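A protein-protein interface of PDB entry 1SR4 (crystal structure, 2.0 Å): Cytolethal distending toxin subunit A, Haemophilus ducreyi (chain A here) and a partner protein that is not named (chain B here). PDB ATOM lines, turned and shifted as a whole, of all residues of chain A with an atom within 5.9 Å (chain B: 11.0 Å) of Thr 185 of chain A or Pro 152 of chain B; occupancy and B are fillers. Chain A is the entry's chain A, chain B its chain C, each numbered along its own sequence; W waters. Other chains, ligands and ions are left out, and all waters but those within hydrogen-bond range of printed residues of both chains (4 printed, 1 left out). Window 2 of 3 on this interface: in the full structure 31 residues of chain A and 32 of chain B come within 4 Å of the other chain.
The backbone carbonyl oxygen (O) of Gln 66 of chain A is in hydrogen-bond range of the guanidinium group (NH2) of Arg 23 of chain B.
The side-chain amide nitrogen (NE2) of Gln 66 of chain A is in hydrogen-bond range of the backbone carbonyl oxygen (O) of Gly 151 of chain B, at 3.1 Å.
NZ of Lys 154 of chain B lies within salt-bridge range of OD2 of Asp 148 of chain A (3.8 Å).
Printed residues of chain A that touch a printed residue of chain B: Gln 66, Asp 148, Ser 149, Thr 185 and Thr 192.
Of the 19 printed residues of chain B, 9 touch a printed residue of chain A.
Hydrophobic or aromatic side chains of chain B that line the printed part of chain A: Pro 148, Pro 149, Phe 150, Pro 152 and Leu 156.
Among the printed residues, 11 pairs touch across the chains.
Water W3 lies within hydrogen-bond range of the side-chain hydroxyl (OG1) of Thr 185 of chain A (2.6 Å) and the backbone carbonyl oxygen (O) of Ser 153 of chain B (3.2 Å).
Water W2 lies within hydrogen-bond range of the backbone carbonyl oxygen of Ser 153 of chain B and the backbone carbonyl oxygen of Gly 183 of chain A.
Water W1 lies within hydrogen-bond range of OG of Ser 149 of chain A (2.8 Å) and O of Pro 149 of chain B (2.9 Å).
Water W4 lies within hydrogen-bond range of the backbone carbonyl oxygen (O) of Gly 151 of chain B (2.8 Å), the side-chain hydroxyl (OG) of Ser 153 of chain B (2.9 Å) and the side-chain hydroxyl (OG1) of Thr 192 of chain A (3.1 Å).
The side-chain carboxylate (OD2) of Asp 190 of chain A lies within hydrogen-bond range of the side-chain amide nitrogen (NE2) of Gln 66 of chain A, 2.8 Å away.
NE2 of Gln 66 of chain A lies within hydrogen-bond range of OG1 of Thr 192 of chain A (2.9 Å).
OD1 of Asp 190 of chain A sits at hydrogen-bond distance from OG1 of Thr 192 of chain A (2.7 Å).
The side-chain hydroxyl of Ser 21 of chain B sits at hydrogen-bond distance from the backbone NH of Phe 150 of chain B, at 2.9 Å.
The backbone carbonyl oxygen (O) of Phe 150 of chain B lies within hydrogen-bond range of a ring nitrogen (NE2) of His 45 of chain B (2.6 Å).
Among the printed residues, pairs that only touch across the chains: Gln 66 of chain A with Phe 150 of chain B, Asp 148 of chain A with Ser 153 of chain B, Asp 148 of chain A with Leu 156 of chain B, Ser 149 of chain A with Pro 148 of chain B, Ser 149 of chain A with Pro 149 of chain B, Ser 149 of chain A with Ser 153 of chain B, Thr 185 of chain A with Pro 152 of chain B and Thr 192 of chain A with Ser 153 of chain B.
Pro 152 of chain B touches just one residue of chain A: Thr 185.
No residue of chain B comes within 4 Å of Asp 190 of chain A.
Printed residues of chain A within 4 Å of Gly 151 of chain B: Gln 66 (3.1 Å).
Of the printed residues of chain A, Pro 148 of chain B touches Ser 149.
The nearest printed residue of chain B that does not touch Gln 66 of chain A is Pro 149 of chain B (4.4 Å).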
ATOM      1  N   GLN A  66      27.851  -4.910 -28.816  1.00  0.00           N
ATOM      2  CA  GLN A  66      27.931  -5.985 -27.831  1.00  0.00           C
ATOM      3  C   GLN A  66      28.799  -5.646 -26.625  1.00  0.00           C
ATOM      4  O   GLN A  66      28.750  -6.334 -25.593  1.00  0.00           O
ATOM      5  CB  GLN A  66      28.434  -7.253 -28.505  1.00  0.00           C
ATOM      6  CG  GLN A  66      27.487  -7.746 -29.589  1.00  0.00           C
ATOM      7  CD  GLN A  66      27.393  -9.240 -29.579  1.00  0.00           C
ATOM      8  OE1 GLN A  66      26.604  -9.814 -28.829  1.00  0.00           O
ATOM      9  NE2 GLN A  66      28.219  -9.891 -30.391  1.00  0.00           N
ATOM     10  N   ASP A 148      19.655 -14.695 -35.438  1.00  0.00           N
ATOM     11  CA  ASP A 148      18.883 -15.638 -34.645  1.00  0.00           C
ATOM     12  C   ASP A 148      18.936 -15.440 -33.135  1.00  0.00           C
ATOM     13  O   ASP A 148      18.336 -16.212 -32.392  1.00  0.00           O
ATOM     14  CB  ASP A 148      19.220 -17.088 -34.996  1.00  0.00           C
ATOM     15  CG  ASP A 148      20.690 -17.406 -34.886  1.00  0.00           C
ATOM     16  OD1 ASP A 148      21.470 -16.604 -34.320  1.00  0.00           O
ATOM     17  OD2 ASP A 148      21.059 -18.495 -35.374  1.00  0.00           O
ATOM     18  N   SER A 149      19.630 -14.405 -32.671  1.00  0.00           N
ATOM     19  CA  SER A 149      19.660 -14.135 -31.231  1.00  0.00           C
ATOM     20  C   SER A 149      18.726 -12.973 -30.934  1.00  0.00           C
ATOM     21  O   SER A 149      18.494 -12.638 -29.771  1.00  0.00           O
ATOM     22  CB  SER A 149      21.067 -13.766 -30.765  1.00  0.00           C
ATOM     23  OG  SER A 149      21.427 -12.488 -31.251  1.00  0.00           O
ATOM     24  N   GLY A 183      28.514 -10.859 -40.784  1.00  0.00           N
ATOM     25  CA  GLY A 183      27.952 -11.151 -39.475  1.00  0.00           C
ATOM     26  C   GLY A 183      28.982 -11.624 -38.468  1.00  0.00           C
ATOM     27  O   GLY A 183      28.672 -12.359 -37.528  1.00  0.00           O
ATOM     28  N   ALA A 184      30.221 -11.196 -38.650  1.00  0.00           N
ATOM     29  CA  ALA A 184      31.276 -11.594 -37.733  1.00  0.00           C
ATOM     30  C   ALA A 184      30.993 -11.065 -36.323  1.00  0.00           C
ATOM     31  O   ALA A 184      30.358 -10.030 -36.161  1.00  0.00           O
ATOM     32  CB  ALA A 184      32.615 -11.061 -38.223  1.00  0.00           C
ATOM     33  N   THR A 185      31.443 -11.808 -35.316  1.00  0.00           N
ATOM     34  CA  THR A 185      31.298 -11.405 -33.920  1.00  0.00           C
ATOM     35  C   THR A 185      32.622 -11.713 -33.214  1.00  0.00           C
ATOM     36  O   THR A 185      32.678 -12.538 -32.318  1.00  0.00           O
ATOM     37  CB  THR A 185      30.136 -12.155 -33.196  1.00  0.00           C
ATOM     38  OG1 THR A 185      30.327 -13.570 -33.311  1.00  0.00           O
ATOM     39  CG2 THR A 185      28.776 -11.769 -33.803  1.00  0.00           C
ATOM     40  N   GLU A 186      33.682 -11.037 -33.640  1.00  0.00           N
ATOM     41  CA  GLU A 186      35.012 -11.227 -33.069  1.00  0.00           C
ATOM     42  C   GLU A 186      35.408 -10.029 -32.206  1.00  0.00           C
ATOM     43  O   GLU A 186      34.849  -8.938 -32.342  1.00  0.00           O
ATOM     44  CB  GLU A 186      36.059 -11.377 -34.185  1.00  0.00           C
ATOM     45  CG  GLU A 186      35.847 -12.547 -35.138  1.00  0.00           C
ATOM     46  CD  GLU A 186      35.799 -13.889 -34.418  1.00  0.00           C
ATOM     47  OE1 GLU A 186      36.698 -14.162 -33.592  1.00  0.00           O
ATOM     48  OE2 GLU A 186      34.865 -14.675 -34.678  1.00  0.00           O
ATOM     49  N   PRO A 187      36.408 -10.214 -31.328  1.00  0.00           N
ATOM     50  CA  PRO A 187      36.903  -9.155 -30.434  1.00  0.00           C
ATOM     51  C   PRO A 187      37.314  -7.882 -31.172  1.00  0.00           C
ATOM     52  O   PRO A 187      37.128  -6.773 -30.663  1.00  0.00           O
ATOM     53  CB  PRO A 187      38.086  -9.828 -29.743  1.00  0.00           C
ATOM     54  CG  PRO A 187      37.591 -11.246 -29.604  1.00  0.00           C
ATOM     55  CD  PRO A 187      37.023 -11.512 -30.984  1.00  0.00           C
ATOM     56  N   ARG A 189      36.311  -7.246 -34.470  1.00  0.00           N
ATOM     57  CA  ARG A 189      35.396  -6.955 -35.569  1.00  0.00           C
ATOM     58  C   ARG A 189      34.048  -7.628 -35.305  1.00  0.00           C
ATOM     59  O   ARG A 189      33.943  -8.854 -35.336  1.00  0.00           O
ATOM     60  CB  ARG A 189      36.019  -7.481 -36.871  1.00  0.00           C
ATOM     61  CG  ARG A 189      35.159  -7.307 -38.113  1.00  0.00           C
ATOM     62  CD  ARG A 189      35.925  -7.675 -39.401  1.00  0.00           C
ATOM     63  NE  ARG A 189      35.150  -7.298 -40.584  1.00  0.00           N
ATOM     64  CZ  ARG A 189      34.184  -8.038 -41.112  1.00  0.00           C
ATOM     65  NH1 ARG A 189      33.882  -9.213 -40.574  1.00  0.00           N
ATOM     66  NH2 ARG A 189      33.481  -7.584 -42.152  1.00  0.00           N
ATOM     67  N   ASP A 190      33.026  -6.823 -35.040  1.00  0.00           N
ATOM     68  CA  ASP A 190      31.695  -7.355 -34.741  1.00  0.00           C
ATOM     69  C   ASP A 190      30.697  -6.525 -35.543  1.00  0.00           C
ATOM     70  O   ASP A 190      30.937  -5.338 -35.801  1.00  0.00           O
ATOM     71  CB  ASP A 190      31.430  -7.203 -33.247  1.00  0.00           C
ATOM     72  CG  ASP A 190      30.281  -8.069 -32.739  1.00  0.00           C
ATOM     73  OD1 ASP A 190      29.248  -8.251 -33.421  1.00  0.00           O
ATOM     74  OD2 ASP A 190      30.401  -8.546 -31.600  1.00  0.00           O
ATOM     75  N   GLN A 191      29.599  -7.144 -35.966  1.00  0.00           N
ATOM     76  CA  GLN A 191      28.605  -6.409 -36.732  1.00  0.00           C
ATOM     77  C   GLN A 191      27.228  -6.517 -36.094  1.00  0.00           C
ATOM     78  O   GLN A 191      26.227  -6.154 -36.720  1.00  0.00           O
ATOM     79  CB  GLN A 191      28.541  -6.911 -38.185  1.00  0.00           C
ATOM     80  CG  GLN A 191      29.839  -6.742 -38.968  1.00  0.00           C
ATOM     81  CD  GLN A 191      29.704  -7.175 -40.421  1.00  0.00           C
ATOM     82  OE1 GLN A 191      29.021  -8.159 -40.724  1.00  0.00           O
ATOM     83  NE2 GLN A 191      30.366  -6.450 -41.327  1.00  0.00           N
ATOM     84  N   THR A 192      27.154  -7.009 -34.858  1.00  0.00           N
ATOM     85  CA  THR A 192      25.835  -7.114 -34.231  1.00  0.00           C
ATOM     86  C   THR A 192      25.577  -5.951 -33.283  1.00  0.00           C
ATOM     87  O   THR A 192      26.445  -5.546 -32.503  1.00  0.00           O
ATOM     88  CB  THR A 192      25.632  -8.466 -33.471  1.00  0.00           C
ATOM     89  OG1 THR A 192      26.740  -8.721 -32.624  1.00  0.00           O
ATOM     90  CG2 THR A 192      25.527  -9.623 -34.449  1.00  0.00           C
ATOM     91  N   ARG B  19      15.719 -16.214 -24.357  1.00  0.00           N
ATOM     92  CA  ARG B  19      17.084 -16.021 -23.893  1.00  0.00           C
ATOM     93  C   ARG B  19      17.391 -14.517 -23.907  1.00  0.00           C
ATOM     94  O   ARG B  19      17.033 -13.831 -24.856  1.00  0.00           O
ATOM     95  CB  ARG B  19      18.050 -16.738 -24.835  1.00  0.00           C
ATOM     96  CG  ARG B  19      19.475 -16.814 -24.331  1.00  0.00           C
ATOM     97  CD  ARG B  19      19.586 -17.875 -23.249  1.00  0.00           C
ATOM     98  NE  ARG B  19      19.319 -19.207 -23.788  1.00  0.00           N
ATOM     99  CZ  ARG B  19      20.219 -19.949 -24.426  1.00  0.00           C
ATOM    100  NH1 ARG B  19      21.459 -19.494 -24.612  1.00  0.00           N
ATOM    101  NH2 ARG B  19      19.883 -21.156 -24.871  1.00  0.00           N
ATOM    102  N   SER B  21      20.203 -11.132 -22.172  1.00  0.00           N
ATOM    103  CA  SER B  21      21.357 -10.728 -21.394  1.00  0.00           C
ATOM    104  C   SER B  21      20.729  -9.537 -20.657  1.00  0.00           C
ATOM    105  O   SER B  21      19.921  -8.807 -21.232  1.00  0.00           O
ATOM    106  CB  SER B  21      22.551 -10.287 -22.241  1.00  0.00           C
ATOM    107  OG  SER B  21      23.424 -11.387 -22.489  1.00  0.00           O
ATOM    108  N   ARG B  23      21.464  -6.083 -18.826  1.00  0.00           N
ATOM    109  CA  ARG B  23      22.490  -5.059 -18.713  1.00  0.00           C
ATOM    110  C   ARG B  23      22.042  -3.782 -18.002  1.00  0.00           C
ATOM    111  O   ARG B  23      20.939  -3.296 -18.209  1.00  0.00           O
ATOM    112  CB  ARG B  23      22.995  -4.641 -20.107  1.00  0.00           C
ATOM    113  CG  ARG B  23      23.686  -5.718 -20.931  1.00  0.00           C
ATOM    114  CD  ARG B  23      24.048  -5.166 -22.299  1.00  0.00           C
ATOM    115  NE  ARG B  23      24.637  -6.159 -23.191  1.00  0.00           N
ATOM    116  CZ  ARG B  23      25.942  -6.271 -23.446  1.00  0.00           C
ATOM    117  NH1 ARG B  23      26.813  -5.444 -22.873  1.00  0.00           N
ATOM    118  NH2 ARG B  23      26.377  -7.211 -24.283  1.00  0.00           N
ATOM    119  N   HIS B  39      34.799 -16.248 -19.117  1.00  0.00           N
ATOM    120  CA  HIS B  39      35.143 -15.892 -20.488  1.00  0.00           C
ATOM    121  C   HIS B  39      34.318 -16.663 -21.515  1.00  0.00           C
ATOM    122  O   HIS B  39      34.533 -16.535 -22.714  1.00  0.00           O
ATOM    123  CB  HIS B  39      36.651 -16.082 -20.725  1.00  0.00           C
ATOM    124  CG  HIS B  39      37.516 -15.311 -19.768  1.00  0.00           C
ATOM    125  ND1 HIS B  39      37.304 -13.978 -19.475  1.00  0.00           N
ATOM    126  CD2 HIS B  39      38.590 -15.689 -19.028  1.00  0.00           C
ATOM    127  CE1 HIS B  39      38.205 -13.570 -18.597  1.00  0.00           C
ATOM    128  NE2 HIS B  39      38.998 -14.588 -18.309  1.00  0.00           N
ATOM    129  N   ASN B  40      33.365 -17.460 -21.038  1.00  0.00           N
ATOM    130  CA  ASN B  40      32.473 -18.221 -21.922  1.00  0.00           C
ATOM    131  C   ASN B  40      31.234 -17.332 -22.054  1.00  0.00           C
ATOM    132  O   ASN B  40      30.743 -16.811 -21.053  1.00  0.00           O
ATOM    133  CB  ASN B  40      32.085 -19.547 -21.281  1.00  0.00           C
ATOM    134  CG  ASN B  40      31.147 -20.360 -22.148  1.00  0.00           C
ATOM    135  OD1 ASN B  40      30.245 -19.814 -22.787  1.00  0.00           O
ATOM    136  ND2 ASN B  40      31.341 -21.678 -22.160  1.00  0.00           N
ATOM    137  N   TYR B  41      30.715 -17.153 -23.266  1.00  0.00           N
ATOM    138  CA  TYR B  41      29.577 -16.261 -23.406  1.00  0.00           C
ATOM    139  C   TYR B  41      28.308 -16.675 -22.650  1.00  0.00           C
ATOM    140  O   TYR B  41      27.516 -15.809 -22.243  1.00  0.00           O
ATOM    141  CB  TYR B  41      29.305 -15.958 -24.897  1.00  0.00           C
ATOM    142  CG  TYR B  41      28.765 -17.076 -25.773  1.00  0.00           C
ATOM    143  CD1 TYR B  41      27.396 -17.328 -25.844  1.00  0.00           C
ATOM    144  CD2 TYR B  41      29.616 -17.817 -26.603  1.00  0.00           C
ATOM    145  CE1 TYR B  41      26.876 -18.275 -26.720  1.00  0.00           C
ATOM    146  CE2 TYR B  41      29.106 -18.775 -27.487  1.00  0.00           C
ATOM    147  CZ  TYR B  41      27.735 -18.993 -27.541  1.00  0.00           C
ATOM    148  OH  TYR B  41      27.204 -19.900 -28.436  1.00  0.00           O
ATOM    149  N   LEU B  42      28.117 -17.969 -22.419  1.00  0.00           N
ATOM    150  CA  LEU B  42      26.928 -18.403 -21.687  1.00  0.00           C
ATOM    151  C   LEU B  42      26.876 -17.830 -20.268  1.00  0.00           C
ATOM    152  O   LEU B  42      25.835 -17.880 -19.613  1.00  0.00           O
ATOM    153  CB  LEU B  42      26.827 -19.941 -21.640  1.00  0.00           C
ATOM    154  CG  LEU B  42      26.458 -20.639 -22.957  1.00  0.00           C
ATOM    155  CD1 LEU B  42      26.324 -22.140 -22.695  1.00  0.00           C
ATOM    156  CD2 LEU B  42      25.144 -20.076 -23.536  1.00  0.00           C
ATOM    157  N   SER B  43      27.995 -17.288 -19.792  1.00  0.00           N
ATOM    158  CA  SER B  43      28.020 -16.695 -18.468  1.00  0.00           C
ATOM    159  C   SER B  43      27.241 -15.378 -18.458  1.00  0.00           C
ATOM    160  O   SER B  43      26.983 -14.820 -17.390  1.00  0.00           O
ATOM    161  CB  SER B  43      29.459 -16.443 -18.014  1.00  0.00           C
ATOM    162  OG  SER B  43      30.097 -15.491 -18.839  1.00  0.00           O
ATOM    163  N   THR B  44      26.878 -14.879 -19.642  1.00  0.00           N
ATOM    164  CA  THR B  44      26.125 -13.624 -19.738  1.00  0.00           C
ATOM    165  C   THR B  44      24.666 -13.854 -20.126  1.00  0.00           C
ATOM    166  O   THR B  44      23.893 -12.891 -20.259  1.00  0.00           O
ATOM    167  CB  THR B  44      26.724 -12.656 -20.783  1.00  0.00           C
ATOM    168  OG1 THR B  44      26.616 -13.244 -22.087  1.00  0.00           O
ATOM    169  CG2 THR B  44      28.196 -12.357 -20.480  1.00  0.00           C
ATOM    170  N   HIS B  45      24.292 -15.125 -20.297  1.00  0.00           N
ATOM    171  CA  HIS B  45      22.926 -15.496 -20.687  1.00  0.00           C
ATOM    172  C   HIS B  45      22.035 -15.915 -19.524  1.00  0.00           C
ATOM    173  O   HIS B  45      22.499 -16.530 -18.558  1.00  0.00           O
ATOM    174  CB  HIS B  45      22.928 -16.677 -21.674  1.00  0.00           C
ATOM    175  CG  HIS B  45      23.496 -16.360 -23.021  1.00  0.00           C
ATOM    176  ND1 HIS B  45      23.129 -17.050 -24.155  1.00  0.00           N
ATOM    177  CD2 HIS B  45      24.422 -15.453 -23.415  1.00  0.00           C
ATOM    178  CE1 HIS B  45      23.807 -16.586 -25.192  1.00  0.00           C
ATOM    179  NE2 HIS B  45      24.599 -15.618 -24.770  1.00  0.00           N
ATOM    180  N   PRO B 148      19.099  -8.753 -26.309  1.00  0.00           N
ATOM    181  CA  PRO B 148      19.492 -10.018 -26.939  1.00  0.00           C
ATOM    182  C   PRO B 148      20.711 -10.558 -26.169  1.00  0.00           C
ATOM    183  O   PRO B 148      21.507  -9.790 -25.620  1.00  0.00           O
ATOM    184  CB  PRO B 148      19.833  -9.600 -28.376  1.00  0.00           C
ATOM    185  CG  PRO B 148      18.891  -8.415 -28.622  1.00  0.00           C
ATOM    186  CD  PRO B 148      19.009  -7.661 -27.304  1.00  0.00           C
ATOM    187  N   PRO B 149      20.868 -11.888 -26.115  1.00  0.00           N
ATOM    188  CA  PRO B 149      21.995 -12.485 -25.395  1.00  0.00           C
ATOM    189  C   PRO B 149      23.343 -12.242 -26.053  1.00  0.00           C
ATOM    190  O   PRO B 149      23.500 -12.434 -27.269  1.00  0.00           O
ATOM    191  CB  PRO B 149      21.610 -13.954 -25.334  1.00  0.00           C
ATOM    192  CG  PRO B 149      20.823 -14.152 -26.632  1.00  0.00           C
ATOM    193  CD  PRO B 149      19.950 -12.926 -26.629  1.00  0.00           C
ATOM    194  N   PHE B 150      24.317 -11.807 -25.251  1.00  0.00           N
ATOM    195  CA  PHE B 150      25.654 -11.527 -25.756  1.00  0.00           C
ATOM    196  C   PHE B 150      26.315 -12.767 -26.365  1.00  0.00           C
ATOM    197  O   PHE B 150      26.206 -13.883 -25.838  1.00  0.00           O
ATOM    198  CB  PHE B 150      26.565 -11.014 -24.629  1.00  0.00           C
ATOM    199  CG  PHE B 150      28.028 -11.010 -24.997  1.00  0.00           C
ATOM    200  CD1 PHE B 150      28.563  -9.972 -25.764  1.00  0.00           C
ATOM    201  CD2 PHE B 150      28.849 -12.099 -24.658  1.00  0.00           C
ATOM    202  CE1 PHE B 150      29.896 -10.012 -26.205  1.00  0.00           C
ATOM    203  CE2 PHE B 150      30.184 -12.161 -25.088  1.00  0.00           C
ATOM    204  CZ  PHE B 150      30.714 -11.115 -25.868  1.00  0.00           C
ATOM    205  N   GLY B 151      27.038 -12.565 -27.458  1.00  0.00           N
ATOM    206  CA  GLY B 151      27.730 -13.682 -28.069  1.00  0.00           C
ATOM    207  C   GLY B 151      27.541 -13.730 -29.567  1.00  0.00           C
ATOM    208  O   GLY B 151      27.138 -12.743 -30.184  1.00  0.00           O
ATOM    209  N   PRO B 152      27.841 -14.879 -30.183  1.00  0.00           N
ATOM    210  CA  PRO B 152      27.698 -15.056 -31.628  1.00  0.00           C
ATOM    211  C   PRO B 152      26.243 -15.186 -32.015  1.00  0.00           C
ATOM    212  O   PRO B 152      25.388 -15.462 -31.179  1.00  0.00           O
ATOM    213  CB  PRO B 152      28.476 -16.335 -31.889  1.00  0.00           C
ATOM    214  CG  PRO B 152      28.203 -17.137 -30.645  1.00  0.00           C
ATOM    215  CD  PRO B 152      28.360 -16.102 -29.544  1.00  0.00           C
ATOM    216  N   SER B 153      25.956 -14.936 -33.283  1.00  0.00           N
ATOM    217  CA  SER B 153      24.613 -15.074 -33.798  1.00  0.00           C
ATOM    218  C   SER B 153      24.743 -15.108 -35.316  1.00  0.00           C
ATOM    219  O   SER B 153      25.740 -14.667 -35.879  1.00  0.00           O
ATOM    220  CB  SER B 153      23.697 -13.920 -33.341  1.00  0.00           C
ATOM    221  OG  SER B 153      24.001 -12.686 -33.972  1.00  0.00           O
ATOM    222  N   LYS B 154      23.739 -15.641 -35.982  1.00  0.00           N
ATOM    223  CA  LYS B 154      23.792 -15.735 -37.425  1.00  0.00           C
ATOM    224  C   LYS B 154      22.721 -14.883 -38.078  1.00  0.00           C
ATOM    225  O   LYS B 154      21.573 -14.882 -37.640  1.00  0.00           O
ATOM    226  CB  LYS B 154      23.627 -17.206 -37.830  1.00  0.00           C
ATOM    227  CG  LYS B 154      23.229 -17.425 -39.280  1.00  0.00           C
ATOM    228  CD  LYS B 154      23.003 -18.915 -39.584  1.00  0.00           C
ATOM    229  CE  LYS B 154      21.862 -19.495 -38.776  1.00  0.00           C
ATOM    230  NZ  LYS B 154      20.560 -18.832 -39.084  1.00  0.00           N
ATOM    231  N   ILE B 155      23.113 -14.145 -39.108  1.00  0.00           N
ATOM    232  CA  ILE B 155      22.179 -13.334 -39.873  1.00  0.00           C
ATOM    233  C   ILE B 155      21.134 -14.294 -40.450  1.00  0.00           C
ATOM    234  O   ILE B 155      21.493 -15.292 -41.084  1.00  0.00           O
ATOM    235  CB  ILE B 155      22.856 -12.649 -41.082  1.00  0.00           C
ATOM    236  CG1 ILE B 155      23.950 -11.693 -40.619  1.00  0.00           C
ATOM    237  CG2 ILE B 155      21.806 -11.891 -41.903  1.00  0.00           C
ATOM    238  CD1 ILE B 155      23.414 -10.633 -39.718  1.00  0.00           C
ATOM    239  N   LEU B 156      19.853 -13.992 -40.253  1.00  0.00           N
ATOM    240  CA  LEU B 156      18.794 -14.846 -40.782  1.00  0.00           C
ATOM    241  C   LEU B 156      18.688 -14.671 -42.298  1.00  0.00           C
ATOM    242  O   LEU B 156      18.686 -13.549 -42.802  1.00  0.00           O
ATOM    243  CB  LEU B 156      17.448 -14.502 -40.122  1.00  0.00           C
ATOM    244  CG  LEU B 156      17.378 -14.744 -38.612  1.00  0.00           C
ATOM    245  CD1 LEU B 156      16.051 -14.238 -38.063  1.00  0.00           C
ATOM    246  CD2 LEU B 156      17.567 -16.217 -38.322  1.00  0.00           C
HETATM  247  O   HOH W   1      23.431 -11.195 -29.868  1.00  0.00           O
HETATM  248  O   HOH W   2      25.783 -12.107 -36.729  1.00  0.00           O
HETATM  249  O   HOH W   3      28.787 -14.831 -35.004  1.00  0.00           O
HETATM  250  O   HOH W   4      25.368 -11.403 -31.824  1.00  0.00           O
